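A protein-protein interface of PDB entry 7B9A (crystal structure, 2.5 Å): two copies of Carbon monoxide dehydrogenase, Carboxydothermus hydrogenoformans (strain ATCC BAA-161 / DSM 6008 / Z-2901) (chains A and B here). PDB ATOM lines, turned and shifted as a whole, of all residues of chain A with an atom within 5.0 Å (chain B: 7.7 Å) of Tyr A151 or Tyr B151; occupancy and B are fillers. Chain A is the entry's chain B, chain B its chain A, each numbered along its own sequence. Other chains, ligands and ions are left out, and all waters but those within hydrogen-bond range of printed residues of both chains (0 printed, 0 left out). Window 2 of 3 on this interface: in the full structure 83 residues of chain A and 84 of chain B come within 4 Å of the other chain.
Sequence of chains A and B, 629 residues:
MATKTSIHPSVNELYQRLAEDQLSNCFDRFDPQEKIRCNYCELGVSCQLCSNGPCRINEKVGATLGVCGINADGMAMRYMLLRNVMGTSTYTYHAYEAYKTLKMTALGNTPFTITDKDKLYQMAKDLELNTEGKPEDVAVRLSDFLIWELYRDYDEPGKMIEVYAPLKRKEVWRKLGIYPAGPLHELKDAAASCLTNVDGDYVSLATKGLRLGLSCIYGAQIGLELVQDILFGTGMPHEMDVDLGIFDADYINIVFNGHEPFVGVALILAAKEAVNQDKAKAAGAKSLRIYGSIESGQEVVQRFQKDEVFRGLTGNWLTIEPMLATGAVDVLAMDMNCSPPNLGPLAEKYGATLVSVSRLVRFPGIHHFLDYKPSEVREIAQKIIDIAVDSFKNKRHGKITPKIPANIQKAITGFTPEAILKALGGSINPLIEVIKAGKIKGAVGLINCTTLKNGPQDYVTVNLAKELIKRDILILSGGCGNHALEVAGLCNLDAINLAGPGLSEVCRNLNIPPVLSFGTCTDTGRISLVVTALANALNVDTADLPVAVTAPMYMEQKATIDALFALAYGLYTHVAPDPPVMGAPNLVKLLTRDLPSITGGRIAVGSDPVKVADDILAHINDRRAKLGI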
ATOM      1  N   TYR A  96     -16.472  -2.148   6.042  1.00  0.00           N
ATOM      2  CA  TYR A  96     -15.971  -1.333   4.940  1.00  0.00           C
ATOM      3  C   TYR A  96     -16.739  -1.612   3.656  1.00  0.00           C
ATOM      4  O   TYR A  96     -17.079  -0.679   2.912  1.00  0.00           O
ATOM      5  CB  TYR A  96     -14.476  -1.584   4.739  1.00  0.00           C
ATOM      6  CG  TYR A  96     -13.849  -0.686   3.698  1.00  0.00           C
ATOM      7  CD1 TYR A  96     -13.366   0.569   4.041  1.00  0.00           C
ATOM      8  CD2 TYR A  96     -13.743  -1.092   2.374  1.00  0.00           C
ATOM      9  CE1 TYR A  96     -12.795   1.397   3.094  1.00  0.00           C
ATOM     10  CE2 TYR A  96     -13.173  -0.272   1.420  1.00  0.00           C
ATOM     11  CZ  TYR A  96     -12.701   0.971   1.786  1.00  0.00           C
ATOM     12  OH  TYR A  96     -12.135   1.796   0.844  1.00  0.00           O
ATOM     13  N   ILE A 147     -16.371   5.513   7.444  1.00  0.00           N
ATOM     14  CA  ILE A 147     -15.077   5.089   6.923  1.00  0.00           C
ATOM     15  C   ILE A 147     -13.946   5.775   7.682  1.00  0.00           C
ATOM     16  O   ILE A 147     -12.914   5.158   7.974  1.00  0.00           O
ATOM     17  CB  ILE A 147     -15.002   5.354   5.409  1.00  0.00           C
ATOM     18  CG1 ILE A 147     -15.926   4.394   4.659  1.00  0.00           C
ATOM     19  CG2 ILE A 147     -13.579   5.212   4.904  1.00  0.00           C
ATOM     20  CD1 ILE A 147     -15.907   4.572   3.158  1.00  0.00           C
ATOM     21  N   TRP A 148     -14.124   7.055   8.024  1.00  0.00           N
ATOM     22  CA  TRP A 148     -13.152   7.727   8.882  1.00  0.00           C
ATOM     23  C   TRP A 148     -13.041   7.032  10.231  1.00  0.00           C
ATOM     24  O   TRP A 148     -11.941   6.887  10.777  1.00  0.00           O
ATOM     25  CB  TRP A 148     -13.533   9.194   9.074  1.00  0.00           C
ATOM     26  CG  TRP A 148     -12.811   9.838  10.220  1.00  0.00           C
ATOM     27  CD1 TRP A 148     -11.565  10.392  10.196  1.00  0.00           C
ATOM     28  CD2 TRP A 148     -13.291   9.989  11.564  1.00  0.00           C
ATOM     29  NE1 TRP A 148     -11.239  10.881  11.439  1.00  0.00           N
ATOM     30  CE2 TRP A 148     -12.282  10.645  12.296  1.00  0.00           C
ATOM     31  CE3 TRP A 148     -14.475   9.633  12.218  1.00  0.00           C
ATOM     32  CZ2 TRP A 148     -12.420  10.954  13.648  1.00  0.00           C
ATOM     33  CZ3 TRP A 148     -14.611   9.941  13.559  1.00  0.00           C
ATOM     34  CH2 TRP A 148     -13.590  10.595  14.260  1.00  0.00           C
ATOM     35  N   GLU A 149     -14.178   6.611  10.792  1.00  0.00           N
ATOM     36  CA  GLU A 149     -14.149   5.818  12.020  1.00  0.00           C
ATOM     37  C   GLU A 149     -13.307   4.562  11.840  1.00  0.00           C
ATOM     38  O   GLU A 149     -12.587   4.151  12.759  1.00  0.00           O
ATOM     39  CB  GLU A 149     -15.570   5.450  12.450  1.00  0.00           C
ATOM     40  CG  GLU A 149     -16.321   6.550  13.184  1.00  0.00           C
ATOM     41  CD  GLU A 149     -15.891   6.689  14.633  1.00  0.00           C
ATOM     42  OE1 GLU A 149     -16.342   7.647  15.297  1.00  0.00           O
ATOM     43  OE2 GLU A 149     -15.107   5.842  15.111  1.00  0.00           O
ATOM     44  N   LEU A 150     -13.380   3.939  10.660  1.00  0.00           N
ATOM     45  CA  LEU A 150     -12.562   2.755  10.401  1.00  0.00           C
ATOM     46  C   LEU A 150     -11.072   3.085  10.418  1.00  0.00           C
ATOM     47  O   LEU A 150     -10.259   2.290  10.903  1.00  0.00           O
ATOM     48  CB  LEU A 150     -12.948   2.127   9.062  1.00  0.00           C
ATOM     49  CG  LEU A 150     -14.245   1.321   8.987  1.00  0.00           C
ATOM     50  CD1 LEU A 150     -14.464   0.815   7.571  1.00  0.00           C
ATOM     51  CD2 LEU A 150     -14.215   0.161   9.966  1.00  0.00           C
ATOM     52  N   TYR A 151     -10.694   4.250   9.891  1.00  0.00           N
ATOM     53  CA  TYR A 151      -9.292   4.634   9.744  1.00  0.00           C
ATOM     54  C   TYR A 151      -8.750   5.411  10.937  1.00  0.00           C
ATOM     55  O   TYR A 151      -7.605   5.874  10.888  1.00  0.00           O
ATOM     56  CB  TYR A 151      -9.099   5.474   8.481  1.00  0.00           C
ATOM     57  CG  TYR A 151      -9.169   4.700   7.188  1.00  0.00           C
ATOM     58  CD1 TYR A 151      -8.190   3.772   6.858  1.00  0.00           C
ATOM     59  CD2 TYR A 151     -10.199   4.914   6.284  1.00  0.00           C
ATOM     60  CE1 TYR A 151      -8.245   3.067   5.672  1.00  0.00           C
ATOM     61  CE2 TYR A 151     -10.261   4.213   5.094  1.00  0.00           C
ATOM     62  CZ  TYR A 151      -9.283   3.292   4.794  1.00  0.00           C
ATOM     63  OH  TYR A 151      -9.346   2.595   3.611  1.00  0.00           O
ATOM     64  N   ARG A 152      -9.537   5.566  11.997  1.00  0.00           N
ATOM     65  CA  ARG A 152      -9.162   6.442  13.097  1.00  0.00           C
ATOM     66  C   ARG A 152      -7.924   5.921  13.817  1.00  0.00           C
ATOM     67  O   ARG A 152      -7.788   4.720  14.063  1.00  0.00           O
ATOM     68  CB  ARG A 152     -10.331   6.565  14.070  1.00  0.00           C
ATOM     69  CG  ARG A 152     -10.363   7.845  14.869  1.00  0.00           C
ATOM     70  CD  ARG A 152     -11.684   7.960  15.601  1.00  0.00           C
ATOM     71  NE  ARG A 152     -12.078   6.681  16.181  1.00  0.00           N
ATOM     72  CZ  ARG A 152     -11.664   6.240  17.365  1.00  0.00           C
ATOM     73  NH1 ARG A 152     -10.843   6.980  18.097  1.00  0.00           N
ATOM     74  NH2 ARG A 152     -12.071   5.062  17.815  1.00  0.00           N
ATOM     75  N   ASP A 153      -7.008   6.833  14.148  1.00  0.00           N
ATOM     76  CA  ASP A 153      -5.817   6.438  14.890  1.00  0.00           C
ATOM     77  C   ASP A 153      -5.915   6.862  16.352  1.00  0.00           C
ATOM     78  O   ASP A 153      -7.007   6.880  16.929  1.00  0.00           O
ATOM     79  CB  ASP A 153      -4.547   7.001  14.239  1.00  0.00           C
ATOM     80  CG  ASP A 153      -4.523   8.516  14.186  1.00  0.00           C
ATOM     81  OD1 ASP A 153      -5.565   9.147  14.463  1.00  0.00           O
ATOM     82  OD2 ASP A 153      -3.452   9.076  13.868  1.00  0.00           O
ATOM     83  N   GLY A 182      -9.312   3.336  15.595  1.00  0.00           N
ATOM     84  CA  GLY A 182     -10.086   2.643  14.597  1.00  0.00           C
ATOM     85  C   GLY A 182      -9.758   1.164  14.612  1.00  0.00           C
ATOM     86  O   GLY A 182      -8.658   0.759  14.999  1.00  0.00           O
ATOM     87  N   LEU A 184      -9.067  -0.857  12.253  1.00  0.00           N
ATOM     88  CA  LEU A 184      -7.940  -1.215  11.397  1.00  0.00           C
ATOM     89  C   LEU A 184      -6.621  -1.039  12.140  1.00  0.00           C
ATOM     90  O   LEU A 184      -5.801  -1.967  12.220  1.00  0.00           O
ATOM     91  CB  LEU A 184      -7.965  -0.365  10.124  1.00  0.00           C
ATOM     92  CG  LEU A 184      -7.387  -0.948   8.830  1.00  0.00           C
ATOM     93  CD1 LEU A 184      -7.952  -2.332   8.557  1.00  0.00           C
ATOM     94  CD2 LEU A 184      -7.670  -0.020   7.651  1.00  0.00           C
ATOM     95  N   HIS A 185      -6.401   0.159  12.690  1.00  0.00           N
ATOM     96  CA  HIS A 185      -5.198   0.417  13.474  1.00  0.00           C
ATOM     97  C   HIS A 185      -5.106  -0.508  14.684  1.00  0.00           C
ATOM     98  O   HIS A 185      -4.015  -0.965  15.040  1.00  0.00           O
ATOM     99  CB  HIS A 185      -5.165   1.878  13.921  1.00  0.00           C
ATOM    100  CG  HIS A 185      -4.455   2.784  12.968  1.00  0.00           C
ATOM    101  ND1 HIS A 185      -3.084   2.787  12.834  1.00  0.00           N
ATOM    102  CD2 HIS A 185      -4.920   3.714  12.101  1.00  0.00           C
ATOM    103  CE1 HIS A 185      -2.734   3.680  11.926  1.00  0.00           C
ATOM    104  NE2 HIS A 185      -3.830   4.258  11.466  1.00  0.00           N
ATOM    105  N   THR B  92       4.126  -1.925   8.657  1.00  0.00           N
ATOM    106  CA  THR B  92       3.168  -0.836   8.480  1.00  0.00           C
ATOM    107  C   THR B  92       3.160   0.095   9.687  1.00  0.00           C
ATOM    108  O   THR B  92       3.017   1.313   9.538  1.00  0.00           O
ATOM    109  CB  THR B  92       1.772  -1.408   8.229  1.00  0.00           C
ATOM    110  OG1 THR B  92       1.802  -2.249   7.070  1.00  0.00           O
ATOM    111  CG2 THR B  92       0.761  -0.293   8.008  1.00  0.00           C
ATOM    112  N   TYR B  96       3.942   4.019   9.331  1.00  0.00           N
ATOM    113  CA  TYR B  96       2.986   5.028   9.773  1.00  0.00           C
ATOM    114  C   TYR B  96       3.612   5.963  10.797  1.00  0.00           C
ATOM    115  O   TYR B  96       3.427   7.186  10.726  1.00  0.00           O
ATOM    116  CB  TYR B  96       1.740   4.354  10.349  1.00  0.00           C
ATOM    117  CG  TYR B  96       0.619   5.315  10.670  1.00  0.00           C
ATOM    118  CD1 TYR B  96      -0.236   5.769   9.675  1.00  0.00           C
ATOM    119  CD2 TYR B  96       0.414   5.769  11.967  1.00  0.00           C
ATOM    120  CE1 TYR B  96      -1.261   6.648   9.960  1.00  0.00           C
ATOM    121  CE2 TYR B  96      -0.610   6.649  12.263  1.00  0.00           C
ATOM    122  CZ  TYR B  96      -1.445   7.084  11.255  1.00  0.00           C
ATOM    123  OH  TYR B  96      -2.468   7.960  11.541  1.00  0.00           O
ATOM    124  N   ASP B 144       1.411  12.973   3.873  1.00  0.00           N
ATOM    125  CA  ASP B 144       0.014  12.647   3.597  1.00  0.00           C
ATOM    126  C   ASP B 144      -0.111  11.652   2.448  1.00  0.00           C
ATOM    127  O   ASP B 144      -0.945  10.739   2.497  1.00  0.00           O
ATOM    128  CB  ASP B 144      -0.779  13.920   3.304  1.00  0.00           C
ATOM    129  CG  ASP B 144      -1.148  14.677   4.566  1.00  0.00           C
ATOM    130  OD1 ASP B 144      -1.268  14.034   5.631  1.00  0.00           O
ATOM    131  OD2 ASP B 144      -1.319  15.912   4.495  1.00  0.00           O
ATOM    132  N   PHE B 145       0.723  11.794   1.414  1.00  0.00           N
ATOM    133  CA  PHE B 145       0.628  10.879   0.279  1.00  0.00           C
ATOM    134  C   PHE B 145       1.049   9.466   0.663  1.00  0.00           C
ATOM    135  O   PHE B 145       0.429   8.489   0.228  1.00  0.00           O
ATOM    136  CB  PHE B 145       1.472  11.384  -0.890  1.00  0.00           C
ATOM    137  CG  PHE B 145       1.386  10.511  -2.109  1.00  0.00           C
ATOM    138  CD1 PHE B 145       0.324  10.636  -2.989  1.00  0.00           C
ATOM    139  CD2 PHE B 145       2.355   9.556  -2.366  1.00  0.00           C
ATOM    140  CE1 PHE B 145       0.235   9.831  -4.106  1.00  0.00           C
ATOM    141  CE2 PHE B 145       2.272   8.748  -3.482  1.00  0.00           C
ATOM    142  CZ  PHE B 145       1.210   8.887  -4.352  1.00  0.00           C
ATOM    143  N   LEU B 146       2.098   9.330   1.475  1.00  0.00           N
ATOM    144  CA  LEU B 146       2.520   7.995   1.886  1.00  0.00           C
ATOM    145  C   LEU B 146       1.533   7.376   2.871  1.00  0.00           C
ATOM    146  O   LEU B 146       1.329   6.155   2.860  1.00  0.00           O
ATOM    147  CB  LEU B 146       3.929   8.056   2.472  1.00  0.00           C
ATOM    148  CG  LEU B 146       4.986   8.521   1.464  1.00  0.00           C
ATOM    149  CD1 LEU B 146       6.327   8.746   2.135  1.00  0.00           C
ATOM    150  CD2 LEU B 146       5.119   7.528   0.318  1.00  0.00           C
ATOM    151  N   ILE B 147       0.884   8.196   3.701  1.00  0.00           N
ATOM    152  CA  ILE B 147      -0.195   7.679   4.539  1.00  0.00           C
ATOM    153  C   ILE B 147      -1.348   7.182   3.673  1.00  0.00           C
ATOM    154  O   ILE B 147      -1.951   6.137   3.950  1.00  0.00           O
ATOM    155  CB  ILE B 147      -0.655   8.752   5.544  1.00  0.00           C
ATOM    156  CG1 ILE B 147       0.432   8.993   6.594  1.00  0.00           C
ATOM    157  CG2 ILE B 147      -1.957   8.344   6.212  1.00  0.00           C
ATOM    158  CD1 ILE B 147       0.081  10.067   7.599  1.00  0.00           C
ATOM    159  N   TRP B 148      -1.665   7.915   2.602  1.00  0.00           N
ATOM    160  CA  TRP B 148      -2.681   7.449   1.662  1.00  0.00           C
ATOM    161  C   TRP B 148      -2.268   6.133   1.013  1.00  0.00           C
ATOM    162  O   TRP B 148      -3.100   5.237   0.822  1.00  0.00           O
ATOM    163  CB  TRP B 148      -2.940   8.517   0.600  1.00  0.00           C
ATOM    164  CG  TRP B 148      -3.720   8.023  -0.581  1.00  0.00           C
ATOM    165  CD1 TRP B 148      -5.078   7.968  -0.703  1.00  0.00           C
ATOM    166  CD2 TRP B 148      -3.186   7.521  -1.813  1.00  0.00           C
ATOM    167  NE1 TRP B 148      -5.423   7.460  -1.932  1.00  0.00           N
ATOM    168  CE2 TRP B 148      -4.279   7.178  -2.633  1.00  0.00           C
ATOM    169  CE3 TRP B 148      -1.890   7.328  -2.302  1.00  0.00           C
ATOM    170  CZ2 TRP B 148      -4.117   6.653  -3.914  1.00  0.00           C
ATOM    171  CZ3 TRP B 148      -1.731   6.805  -3.574  1.00  0.00           C
ATOM    172  CH2 TRP B 148      -2.838   6.475  -4.364  1.00  0.00           C
ATOM    173  N   GLU B 149      -0.989   6.007   0.653  1.00  0.00           N
ATOM    174  CA  GLU B 149      -0.477   4.736   0.145  1.00  0.00           C
ATOM    175  C   GLU B 149      -0.694   3.617   1.155  1.00  0.00           C
ATOM    176  O   GLU B 149      -0.996   2.477   0.779  1.00  0.00           O
ATOM    177  CB  GLU B 149       1.009   4.863  -0.199  1.00  0.00           C
ATOM    178  CG  GLU B 149       1.300   5.586  -1.504  1.00  0.00           C
ATOM    179  CD  GLU B 149       1.035   4.723  -2.725  1.00  0.00           C
ATOM    180  OE1 GLU B 149       1.057   5.262  -3.850  1.00  0.00           O
ATOM    181  OE2 GLU B 149       0.810   3.505  -2.559  1.00  0.00           O
ATOM    182  N   LEU B 150      -0.527   3.922   2.444  1.00  0.00           N
ATOM    183  CA  LEU B 150      -0.856   2.950   3.481  1.00  0.00           C
ATOM    184  C   LEU B 150      -2.344   2.609   3.472  1.00  0.00           C
ATOM    185  O   LEU B 150      -2.725   1.451   3.674  1.00  0.00           O
ATOM    186  CB  LEU B 150      -0.451   3.480   4.859  1.00  0.00           C
ATOM    187  CG  LEU B 150       1.023   3.495   5.261  1.00  0.00           C
ATOM    188  CD1 LEU B 150       1.178   4.174   6.613  1.00  0.00           C
ATOM    189  CD2 LEU B 150       1.575   2.086   5.315  1.00  0.00           C
ATOM    190  N   TYR B 151      -3.197   3.605   3.234  1.00  0.00           N
ATOM    191  CA  TYR B 151      -4.642   3.459   3.380  1.00  0.00           C
ATOM    192  C   TYR B 151      -5.346   2.956   2.124  1.00  0.00           C
ATOM    193  O   TYR B 151      -6.570   2.787   2.157  1.00  0.00           O
ATOM    194  CB  TYR B 151      -5.272   4.795   3.788  1.00  0.00           C
ATOM    195  CG  TYR B 151      -4.992   5.238   5.206  1.00  0.00           C
ATOM    196  CD1 TYR B 151      -4.365   4.396   6.113  1.00  0.00           C
ATOM    197  CD2 TYR B 151      -5.367   6.503   5.639  1.00  0.00           C
ATOM    198  CE1 TYR B 151      -4.114   4.804   7.409  1.00  0.00           C
ATOM    199  CE2 TYR B 151      -5.122   6.918   6.929  1.00  0.00           C
ATOM    200  CZ  TYR B 151      -4.495   6.066   7.812  1.00  0.00           C
ATOM    201  OH  TYR B 151      -4.250   6.483   9.100  1.00  0.00           O
ATOM    202  N   ARG B 152      -4.622   2.722   1.028  1.00  0.00           N
ATOM    203  CA  ARG B 152      -5.268   2.377  -0.234  1.00  0.00           C
ATOM    204  C   ARG B 152      -6.121   1.122  -0.098  1.00  0.00           C
ATOM    205  O   ARG B 152      -5.724   0.141   0.536  1.00  0.00           O
ATOM    206  CB  ARG B 152      -4.227   2.167  -1.332  1.00  0.00           C
ATOM    207  CG  ARG B 152      -3.704   3.439  -1.965  1.00  0.00           C
ATOM    208  CD  ARG B 152      -3.046   3.139  -3.302  1.00  0.00           C
ATOM    209  NE  ARG B 152      -2.089   2.037  -3.218  1.00  0.00           N
ATOM    210  CZ  ARG B 152      -2.293   0.824  -3.728  1.00  0.00           C
ATOM    211  NH1 ARG B 152      -3.423   0.553  -4.367  1.00  0.00           N
ATOM    212  NH2 ARG B 152      -1.367  -0.115  -3.601  1.00  0.00           N
ATOM    213  N   ASP B 153      -7.303   1.158  -0.708  1.00  0.00           N
ATOM    214  CA  ASP B 153      -8.212   0.025  -0.682  1.00  0.00           C
ATOM    215  C   ASP B 153      -7.996  -0.834  -1.928  1.00  0.00           C
ATOM    216  O   ASP B 153      -7.103  -0.581  -2.741  1.00  0.00           O
ATOM    217  CB  ASP B 153      -9.658   0.503  -0.550  1.00  0.00           C
ATOM    218  CG  ASP B 153     -10.240   0.984  -1.866  1.00  0.00           C
ATOM    219  OD1 ASP B 153      -9.517   1.648  -2.639  1.00  0.00           O
ATOM    220  OD2 ASP B 153     -11.426   0.691  -2.128  1.00  0.00           O
ATOM    221  N   TYR B 154      -8.832  -1.862  -2.091  1.00  0.00           N
ATOM    222  CA  TYR B 154      -8.642  -2.846  -3.148  1.00  0.00           C
ATOM    223  C   TYR B 154      -8.829  -2.268  -4.546  1.00  0.00           C
ATOM    224  O   TYR B 154      -8.313  -2.841  -5.512  1.00  0.00           O
ATOM    225  CB  TYR B 154      -9.610  -4.010  -2.930  1.00  0.00           C
ATOM    226  CG  TYR B 154      -9.365  -5.205  -3.818  1.00  0.00           C
ATOM    227  CD1 TYR B 154      -8.443  -6.180  -3.461  1.00  0.00           C
ATOM    228  CD2 TYR B 154     -10.066  -5.368  -5.006  1.00  0.00           C
ATOM    229  CE1 TYR B 154      -8.218  -7.276  -4.266  1.00  0.00           C
ATOM    230  CE2 TYR B 154      -9.847  -6.460  -5.818  1.00  0.00           C
ATOM    231  CZ  TYR B 154      -8.922  -7.412  -5.443  1.00  0.00           C
ATOM    232  OH  TYR B 154      -8.700  -8.505  -6.247  1.00  0.00           O
ATOM    233  N   GLU B 156      -8.194   1.064  -5.617  1.00  0.00           N
ATOM    234  CA  GLU B 156      -7.514   2.325  -5.875  1.00  0.00           C
ATOM    235  C   GLU B 156      -6.090   2.059  -6.337  1.00  0.00           C
ATOM    236  O   GLU B 156      -5.301   1.469  -5.582  1.00  0.00           O
ATOM    237  CB  GLU B 156      -7.515   3.202  -4.623  1.00  0.00           C
ATOM    238  CG  GLU B 156      -7.349   4.687  -4.895  1.00  0.00           C
ATOM    239  CD  GLU B 156      -7.584   5.534  -3.657  1.00  0.00           C
ATOM    240  OE1 GLU B 156      -7.667   4.964  -2.549  1.00  0.00           O
ATOM    241  OE2 GLU B 156      -7.693   6.771  -3.796  1.00  0.00           O
ATOM    242  N   ALA B 181      -3.374  -4.010  -2.651  1.00  0.00           N
ATOM    243  CA  ALA B 181      -3.900  -2.741  -2.169  1.00  0.00           C
ATOM    244  C   ALA B 181      -2.908  -2.128  -1.190  1.00  0.00           C
ATOM    245  O   ALA B 181      -1.722  -2.473  -1.204  1.00  0.00           O
ATOM    246  CB  ALA B 181      -5.263  -2.938  -1.507  1.00  0.00           C
ATOM    247  N   GLY B 182      -3.377  -1.220  -0.340  1.00  0.00           N
ATOM    248  CA  GLY B 182      -2.564  -0.721   0.740  1.00  0.00           C
ATOM    249  C   GLY B 182      -2.270  -1.830   1.729  1.00  0.00           C
ATOM    250  O   GLY B 182      -3.054  -2.771   1.884  1.00  0.00           O
ATOM    251  N   PRO B 183      -1.120  -1.751   2.403  1.00  0.00           N
ATOM    252  CA  PRO B 183      -0.781  -2.795   3.385  1.00  0.00           C
ATOM    253  C   PRO B 183      -1.824  -2.978   4.474  1.00  0.00           C
ATOM    254  O   PRO B 183      -2.030  -4.111   4.927  1.00  0.00           O
ATOM    255  CB  PRO B 183       0.565  -2.319   3.957  1.00  0.00           C
ATOM    256  CG  PRO B 183       0.716  -0.894   3.510  1.00  0.00           C
ATOM    257  CD  PRO B 183      -0.027  -0.785   2.222  1.00  0.00           C
ATOM    258  N   LEU B 184      -2.500  -1.908   4.899  1.00  0.00           N
ATOM    259  CA  LEU B 184      -3.554  -2.047   5.902  1.00  0.00           C
ATOM    260  C   LEU B 184      -4.668  -2.959   5.402  1.00  0.00           C
ATOM    261  O   LEU B 184      -4.987  -3.977   6.030  1.00  0.00           O
ATOM    262  CB  LEU B 184      -4.110  -0.672   6.277  1.00  0.00           C
ATOM    263  CG  LEU B 184      -3.353   0.113   7.349  1.00  0.00           C
ATOM    264  CD1 LEU B 184      -4.175   1.300   7.818  1.00  0.00           C
ATOM    265  CD2 LEU B 184      -2.998  -0.790   8.520  1.00  0.00           C
ATOM    266  N   HIS B 185      -5.275  -2.603   4.265  1.00  0.00           N
ATOM    267  CA  HIS B 185      -6.336  -3.428   3.699  1.00  0.00           C
ATOM    268  C   HIS B 185      -5.826  -4.816   3.340  1.00  0.00           C
ATOM    269  O   HIS B 185      -6.557  -5.804   3.464  1.00  0.00           O
ATOM    270  CB  HIS B 185      -6.937  -2.751   2.466  1.00  0.00           C
ATOM    271  CG  HIS B 185      -7.946  -1.694   2.785  1.00  0.00           C
ATOM    272  ND1 HIS B 185      -9.249  -1.987   3.126  1.00  0.00           N
ATOM    273  CD2 HIS B 185      -7.847  -0.345   2.800  1.00  0.00           C
ATOM    274  CE1 HIS B 185      -9.908  -0.863   3.342  1.00  0.00           C
ATOM    275  NE2 HIS B 185      -9.080   0.148   3.150  1.00  0.00           N
ATOM    276  N   LYS B 188      -5.516  -6.839   6.466  1.00  0.00           N
ATOM    277  CA  LYS B 188      -6.890  -7.073   6.899  1.00  0.00           C
ATOM    278  C   LYS B 188      -7.514  -8.231   6.129  1.00  0.00           C
ATOM    279  O   LYS B 188      -8.094  -9.149   6.721  1.00  0.00           O
ATOM    280  CB  LYS B 188      -7.713  -5.794   6.726  1.00  0.00           C
ATOM    281  CG  LYS B 188      -9.173  -5.914   7.139  1.00  0.00           C
ATOM    282  CD  LYS B 188     -10.099  -5.967   5.931  1.00  0.00           C
ATOM    283  CE  LYS B 188     -10.022  -4.687   5.113  1.00  0.00           C
ATOM    284  NZ  LYS B 188     -10.972  -4.704   3.964  1.00  0.00           N
ATOM    285  N   GLY B 219       4.252  -0.578  -0.094  1.00  0.00           N
ATOM    286  CA  GLY B 219       3.326   0.269   0.626  1.00  0.00           C
ATOM    287  C   GLY B 219       3.830   0.683   1.992  1.00  0.00           C
ATOM    288  O   GLY B 219       3.183   1.478   2.676  1.00  0.00           O
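The side-chain hydroxyl of Tyr B151 lies within hydrogen-bond range of a ring nitrogen (NE2) of His A185.
OH of Tyr B96 lies within hydrogen-bond range of OD2 of Asp A153 (2.8 Å).
The side-chain hydroxyl of Tyr A151 sits at hydrogen-bond distance from a ring nitrogen (NE2) of His B185, 2.5 Å away.
The side-chain hydroxyl (OH) of Tyr A96 lies close to the side-chain carboxylate (OD2) of Asp B153 (3.2 Å).
OH of Tyr A151 is in hydrogen-bond range of O of Tyr B151, 3.1 Å away.
OH of Tyr B96 lies close to OH of Tyr B151 (3.4 Å).
N of Glu B156 lies close to OD1 of Asp B153.
A ring nitrogen (ND1) of His B185 is in hydrogen-bond range of the side-chain amino group (NZ) of Lys B188.
Among the printed residues, merely in contact across the chains: Tyr A96 with His B185 (3.7 Å), Leu A184 with Leu B184 (3.7 Å), Leu A184 with Lys B188 (3.9 Å) and His A185 with Tyr B96 (3.7 Å).
Of the printed residues of chain B, Tyr A96 touches Asp B153 and His B185.
Of the printed residues of chain A, Tyr B96 touches Asp A153 (2.8 Å) and His A185 (3.7 Å).
Of the printed residues of chain A, Asp B153 touches Tyr A96 (3.1 Å).
Of the printed residues of chain A, Leu B184 touches Leu A184 (3.7 Å).
Of the printed residues of chain A, Lys B188 touches Leu A184.
The nearest printed residue of chain A that does not touch Tyr B151 is Asp A153 (5.2 Å).
Of the 21 printed residues of chain B, 6 touch a printed residue of chain A.
Hydrophobic or aromatic side chains of chain A within 4 Å of the printed part of chain B: Tyr A96, Tyr A151, Leu A184 and His A185.
Among the printed residues, 9 pairs touch across the chains.
Among the printed residues, no Asp or Glu carboxylate lies within 4 Å of a Lys or Arg side-chain nitrogen of the other chain.
Tyr A96 touches Asp B153, and with the chains exchanged Asp A153 touches Tyr B96.
Tyr A96 touches His B185, and with the chains exchanged His A185 touches Tyr B96.
Tyr A151 touches His B185, and with the chains exchanged His A185 touches Tyr B151.
Leu B184 touches its own counterpart, Leu A184.
Of the 9 pairs that touch across the chains among the printed residues, 8 have their exchanged pair printed and touching as well.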
